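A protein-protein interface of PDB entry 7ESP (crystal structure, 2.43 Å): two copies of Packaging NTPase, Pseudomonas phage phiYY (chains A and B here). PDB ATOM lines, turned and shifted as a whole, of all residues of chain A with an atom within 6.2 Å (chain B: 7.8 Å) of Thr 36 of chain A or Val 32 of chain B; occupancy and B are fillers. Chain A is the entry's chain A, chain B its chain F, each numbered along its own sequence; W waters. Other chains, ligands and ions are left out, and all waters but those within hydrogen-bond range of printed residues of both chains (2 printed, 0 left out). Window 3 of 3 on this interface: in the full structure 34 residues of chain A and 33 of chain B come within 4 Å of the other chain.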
ATOM      1  N   GLU A  34       8.354 -16.006  14.100  1.00  0.00           N
ATOM      2  CA  GLU A  34       8.281 -15.439  12.768  1.00  0.00           C
ATOM      3  C   GLU A  34       9.207 -14.236  12.642  1.00  0.00           C
ATOM      4  O   GLU A  34       9.641 -13.645  13.631  1.00  0.00           O
ATOM      5  CB  GLU A  34       6.847 -15.000  12.463  1.00  0.00           C
ATOM      6  CG  GLU A  34       6.361 -13.940  13.447  1.00  0.00           C
ATOM      7  CD  GLU A  34       4.903 -13.596  13.236  1.00  0.00           C
ATOM      8  OE1 GLU A  34       4.545 -13.046  12.155  1.00  0.00           O
ATOM      9  OE2 GLU A  34       4.118 -13.890  14.166  1.00  0.00           O
ATOM     10  N   ALA A  35       9.435 -13.840  11.395  1.00  0.00           N
ATOM     11  CA  ALA A  35      10.272 -12.690  11.100  1.00  0.00           C
ATOM     12  C   ALA A  35       9.806 -11.439  11.842  1.00  0.00           C
ATOM     13  O   ALA A  35       8.621 -11.100  11.841  1.00  0.00           O
ATOM     14  CB  ALA A  35      10.266 -12.452   9.591  1.00  0.00           C
ATOM     15  N   THR A  36      10.750 -10.740  12.477  1.00  0.00           N
ATOM     16  CA  THR A  36      10.495  -9.391  12.970  1.00  0.00           C
ATOM     17  C   THR A  36      11.366  -8.331  12.306  1.00  0.00           C
ATOM     18  O   THR A  36      11.118  -7.143  12.516  1.00  0.00           O
ATOM     19  CB  THR A  36      10.696  -9.316  14.495  1.00  0.00           C
ATOM     20  OG1 THR A  36      11.943  -9.926  14.838  1.00  0.00           O
ATOM     21  CG2 THR A  36       9.574 -10.042  15.224  1.00  0.00           C
ATOM     22  N   THR A  37      12.380  -8.717  11.536  1.00  0.00           N
ATOM     23  CA  THR A  37      13.233  -7.793  10.804  1.00  0.00           C
ATOM     24  C   THR A  37      13.098  -8.076   9.319  1.00  0.00           C
ATOM     25  O   THR A  37      12.632  -9.141   8.905  1.00  0.00           O
ATOM     26  CB  THR A  37      14.725  -7.919  11.192  1.00  0.00           C
ATOM     27  OG1 THR A  37      15.283  -9.095  10.588  1.00  0.00           O
ATOM     28  CG2 THR A  37      14.913  -8.013  12.692  1.00  0.00           C
ATOM     29  N   GLU A  38      13.520  -7.109   8.516  1.00  0.00           N
ATOM     30  CA  GLU A  38      13.464  -7.287   7.074  1.00  0.00           C
ATOM     31  C   GLU A  38      14.363  -8.435   6.625  1.00  0.00           C
ATOM     32  O   GLU A  38      14.030  -9.167   5.683  1.00  0.00           O
ATOM     33  CB  GLU A  38      13.868  -5.986   6.390  1.00  0.00           C
ATOM     34  CG  GLU A  38      12.763  -4.923   6.365  1.00  0.00           C
ATOM     35  CD  GLU A  38      11.436  -5.448   5.789  1.00  0.00           C
ATOM     36  OE1 GLU A  38      10.389  -5.318   6.474  1.00  0.00           O
ATOM     37  OE2 GLU A  38      11.458  -6.000   4.654  1.00  0.00           O
ATOM     38  N   GLU A  40      15.109 -11.242   8.265  1.00  0.00           N
ATOM     39  CA  GLU A  40      14.327 -12.452   8.524  1.00  0.00           C
ATOM     40  C   GLU A  40      13.126 -12.596   7.582  1.00  0.00           C
ATOM     41  O   GLU A  40      12.712 -13.716   7.287  1.00  0.00           O
ATOM     42  CB  GLU A  40      13.822 -12.454   9.969  1.00  0.00           C
ATOM     43  CG  GLU A  40      14.889 -12.734  10.995  1.00  0.00           C
ATOM     44  CD  GLU A  40      14.528 -12.219  12.377  1.00  0.00           C
ATOM     45  OE1 GLU A  40      15.458 -12.120  13.212  1.00  0.00           O
ATOM     46  OE2 GLU A  40      13.328 -11.919  12.636  1.00  0.00           O
ATOM     47  N   ALA A  41      12.533 -11.486   7.129  1.00  0.00           N
ATOM     48  CA  ALA A  41      11.314 -11.559   6.332  1.00  0.00           C
ATOM     49  C   ALA A  41      11.569 -12.133   4.961  1.00  0.00           C
ATOM     50  O   ALA A  41      10.648 -12.679   4.354  1.00  0.00           O
ATOM     51  CB  ALA A  41      10.659 -10.188   6.174  1.00  0.00           C
ATOM     52  N   LEU A  50       8.434 -14.390   4.908  1.00  0.00           N
ATOM     53  CA  LEU A  50       7.237 -14.075   4.151  1.00  0.00           C
ATOM     54  C   LEU A  50       7.425 -14.261   2.655  1.00  0.00           C
ATOM     55  O   LEU A  50       6.562 -13.831   1.878  1.00  0.00           O
ATOM     56  CB  LEU A  50       6.802 -12.627   4.426  1.00  0.00           C
ATOM     57  CG  LEU A  50       6.072 -12.318   5.741  1.00  0.00           C
ATOM     58  CD1 LEU A  50       7.046 -12.300   6.934  1.00  0.00           C
ATOM     59  CD2 LEU A  50       5.389 -11.006   5.623  1.00  0.00           C
ATOM     60  N   ARG A 111      -1.744 -10.038   3.786  1.00  0.00           N
ATOM     61  CA  ARG A 111      -1.547  -8.705   3.240  1.00  0.00           C
ATOM     62  C   ARG A 111      -0.615  -8.748   2.038  1.00  0.00           C
ATOM     63  O   ARG A 111      -0.886  -8.115   1.012  1.00  0.00           O
ATOM     64  CB  ARG A 111      -1.003  -7.782   4.332  1.00  0.00           C
ATOM     65  CG  ARG A 111      -0.849  -6.339   3.937  1.00  0.00           C
ATOM     66  CD  ARG A 111       0.062  -5.601   4.888  1.00  0.00           C
ATOM     67  NE  ARG A 111       1.442  -5.756   4.450  1.00  0.00           N
ATOM     68  CZ  ARG A 111       2.329  -6.502   5.085  1.00  0.00           C
ATOM     69  NH1 ARG A 111       1.992  -7.133   6.201  1.00  0.00           N
ATOM     70  NH2 ARG A 111       3.551  -6.605   4.611  1.00  0.00           N
ATOM     71  N   VAL B  29      11.124  -3.628  -0.867  1.00  0.00           N
ATOM     72  CA  VAL B  29       9.848  -3.267  -0.269  1.00  0.00           C
ATOM     73  C   VAL B  29       9.844  -3.727   1.182  1.00  0.00           C
ATOM     74  O   VAL B  29      10.200  -4.874   1.478  1.00  0.00           O
ATOM     75  CB  VAL B  29       8.691  -3.892  -1.074  1.00  0.00           C
ATOM     76  CG1 VAL B  29       7.368  -3.750  -0.376  1.00  0.00           C
ATOM     77  CG2 VAL B  29       8.615  -3.247  -2.442  1.00  0.00           C
ATOM     78  N   ALA B  30       9.451  -2.835   2.093  1.00  0.00           N
ATOM     79  CA  ALA B  30       9.348  -3.194   3.506  1.00  0.00           C
ATOM     80  C   ALA B  30       8.174  -4.151   3.709  1.00  0.00           C
ATOM     81  O   ALA B  30       7.036  -3.813   3.367  1.00  0.00           O
ATOM     82  CB  ALA B  30       9.168  -1.939   4.359  1.00  0.00           C
ATOM     83  N   LEU B  31       8.454  -5.331   4.286  1.00  0.00           N
ATOM     84  CA  LEU B  31       7.499  -6.417   4.470  1.00  0.00           C
ATOM     85  C   LEU B  31       6.956  -6.525   5.879  1.00  0.00           C
ATOM     86  O   LEU B  31       5.807  -6.981   6.065  1.00  0.00           O
ATOM     87  CB  LEU B  31       8.141  -7.762   4.109  1.00  0.00           C
ATOM     88  CG  LEU B  31       8.525  -7.921   2.638  1.00  0.00           C
ATOM     89  CD1 LEU B  31       9.199  -9.253   2.378  1.00  0.00           C
ATOM     90  CD2 LEU B  31       7.331  -7.721   1.721  1.00  0.00           C
ATOM     91  N   VAL B  32       7.747  -6.147   6.884  1.00  0.00           N
ATOM     92  CA  VAL B  32       7.320  -6.413   8.248  1.00  0.00           C
ATOM     93  C   VAL B  32       7.581  -5.233   9.181  1.00  0.00           C
ATOM     94  O   VAL B  32       6.871  -5.064  10.175  1.00  0.00           O
ATOM     95  CB  VAL B  32       7.980  -7.702   8.769  1.00  0.00           C
ATOM     96  CG1 VAL B  32       9.453  -7.452   9.048  1.00  0.00           C
ATOM     97  CG2 VAL B  32       7.255  -8.218  10.034  1.00  0.00           C
ATOM     98  N   VAL B  33       8.569  -4.388   8.891  1.00  0.00           N
ATOM     99  CA  VAL B  33       8.872  -3.275   9.788  1.00  0.00           C
ATOM    100  C   VAL B  33       8.227  -2.009   9.237  1.00  0.00           C
ATOM    101  O   VAL B  33       8.487  -1.602   8.103  1.00  0.00           O
ATOM    102  CB  VAL B  33      10.384  -3.108  10.023  1.00  0.00           C
ATOM    103  CG1 VAL B  33      11.124  -2.796   8.746  1.00  0.00           C
ATOM    104  CG2 VAL B  33      10.605  -1.978  10.992  1.00  0.00           C
ATOM    105  N   GLU B  34       7.357  -1.404  10.028  1.00  0.00           N
ATOM    106  CA  GLU B  34       6.623  -0.216   9.629  1.00  0.00           C
ATOM    107  C   GLU B  34       7.017   0.962  10.514  1.00  0.00           C
ATOM    108  O   GLU B  34       7.699   0.810  11.531  1.00  0.00           O
ATOM    109  CB  GLU B  34       5.114  -0.457   9.726  1.00  0.00           C
ATOM    110  CG  GLU B  34       4.676  -0.748  11.138  1.00  0.00           C
ATOM    111  CD  GLU B  34       3.219  -1.184  11.232  1.00  0.00           C
ATOM    112  OE1 GLU B  34       2.976  -2.345  11.674  1.00  0.00           O
ATOM    113  OE2 GLU B  34       2.326  -0.356  10.891  1.00  0.00           O
ATOM    114  N   ALA B  35       6.532   2.139  10.128  1.00  0.00           N
ATOM    115  CA  ALA B  35       6.854   3.372  10.830  1.00  0.00           C
ATOM    116  C   ALA B  35       6.364   3.351  12.269  1.00  0.00           C
ATOM    117  O   ALA B  35       5.215   2.991  12.551  1.00  0.00           O
ATOM    118  CB  ALA B  35       6.248   4.570  10.103  1.00  0.00           C
ATOM    119  N   GLY B  48       7.861   1.592   4.407  1.00  0.00           N
ATOM    120  CA  GLY B  48       7.152   1.375   5.651  1.00  0.00           C
ATOM    121  C   GLY B  48       6.480   2.601   6.203  1.00  0.00           C
ATOM    122  O   GLY B  48       5.932   2.540   7.312  1.00  0.00           O
ATOM    123  N   VAL B 105       3.131  -2.123   4.142  1.00  0.00           N
ATOM    124  CA  VAL B 105       3.062  -2.734   5.468  1.00  0.00           C
ATOM    125  C   VAL B 105       2.439  -1.802   6.504  1.00  0.00           C
ATOM    126  O   VAL B 105       1.919  -2.276   7.518  1.00  0.00           O
ATOM    127  CB  VAL B 105       4.480  -3.159   5.914  1.00  0.00           C
ATOM    128  CG1 VAL B 105       5.400  -1.936   6.048  1.00  0.00           C
ATOM    129  CG2 VAL B 105       4.446  -3.922   7.220  1.00  0.00           C
ATOM    130  N   ALA B 106       2.513  -0.478   6.319  1.00  0.00           N
ATOM    131  CA  ALA B 106       2.038   0.433   7.363  1.00  0.00           C
ATOM    132  C   ALA B 106       0.546   0.230   7.605  1.00  0.00           C
ATOM    133  O   ALA B 106      -0.251   0.191   6.657  1.00  0.00           O
ATOM    134  CB  ALA B 106       2.306   1.884   6.975  1.00  0.00           C
HETATM  135  O   HOH W   1       4.676  -5.152   2.222  1.00  0.00           O
HETATM  136  O   HOH W   2       4.160  -8.431   7.894  1.00  0.00           O
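The guanidinium group (NH2) of Arg 111 of chain A sits at hydrogen-bond distance from the backbone carbonyl oxygen (O) of Leu 31 of chain B (2.7 Å).
OE1 of Glu 38 of chain A sits at hydrogen-bond distance from N of Leu 31 of chain B, 2.9 Å away.
The side-chain carboxylate of Glu 38 of chain A lies within hydrogen-bond range of the backbone NH of Val 32 of chain B, 2.8 Å away.
N of Val 33 of chain B sits at hydrogen-bond distance from OE1 of Glu 38 of chain A, at 3.2 Å.
The backbone NH of Thr 36 of chain A is in hydrogen-bond range of the side-chain carboxylate of Glu 40 of chain A, at 2.8 Å.
OG1 of Thr 37 of chain A is in hydrogen-bond range of N of Glu 40 of chain A, 3.2 Å away.
Val 32 of chain B touches Ala 35 of chain A (CG2 to O, 3.7 Å).
O of Thr 36 of chain A touches CG1 of Val 32 of chain B, at 3.9 Å.
O of Thr 37 of chain A touches CG1 of Val 32 of chain B, 3.6 Å away.
Glu 38 of chain A touches Val 29 of chain B.
Ala 30 of chain B touches Glu 38 of chain A.
Arg 111 of chain A touches Val 105 of chain B (NE to CA, 3.6 Å).
Of the printed residues of chain B, Thr 36 of chain A touches Val 32 (3.9 Å).
Val 32 of chain B touches just these residues of chain A: Ala 35 (3.7 Å), Thr 36 (3.9 Å), Thr 37 (3.6 Å) and Glu 38 (2.8 Å).
Of the printed residues of chain A, Val 105 of chain B touches Arg 111 (3.6 Å).
Of the printed residues of chain B, Glu 38 of chain A touches Val 29 (3.6 Å), Ala 30 (3.7 Å), Leu 31 (2.9 Å), Val 32 (2.8 Å) and Val 33 (3.2 Å).
Of the printed residues of chain A, Ala 30 of chain B touches Glu 38 (3.7 Å).
Of the printed residues of chain A, Val 33 of chain B touches Glu 38 (3.2 Å).
Ala 106 of chain B touches none of the printed residues of chain A.
Ala 35 of chain B touches none of the printed residues of chain A.
The nearest residue of chain B that does not touch Thr 36 of chain A is Val 33 of chain B (4.8 Å).
The nearest residue of chain A that does not touch Val 32 of chain B is Ala 41 of chain A (4.1 Å).
The nearest printed residue of chain B that does not touch Arg 111 of chain A is Ala 30 of chain B (4.6 Å).
Of the 9 printed residues of chain A, 5 touch a printed residue of chain B.
Printed residues of chain A that touch a printed residue of chain B: Ala 35, Thr 36, Thr 37, Glu 38 and Arg 111.
Of the 10 printed residues of chain B, 6 touch a printed residue of chain A.
Printed residues of chain B that touch a printed residue of chain A: Val 29, Ala 30, Leu 31, Val 32, Val 33 and Val 105.
Hydrophobic or aromatic side chains of chain B that line the printed part of chain A: Leu 31, Val 32, Val 33 and Val 105.
Positions printed for both chains: 34 and 35.
Water W2 bridges O of Leu 31 of chain B (2.9 Å) and NH1 of Arg 111 of chain A (3.0 Å).
Water W1 lies within hydrogen-bond range of O of Ala 30 of chain B (2.9 Å) and NH2 of Arg 111 of chain A (3.0 Å).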
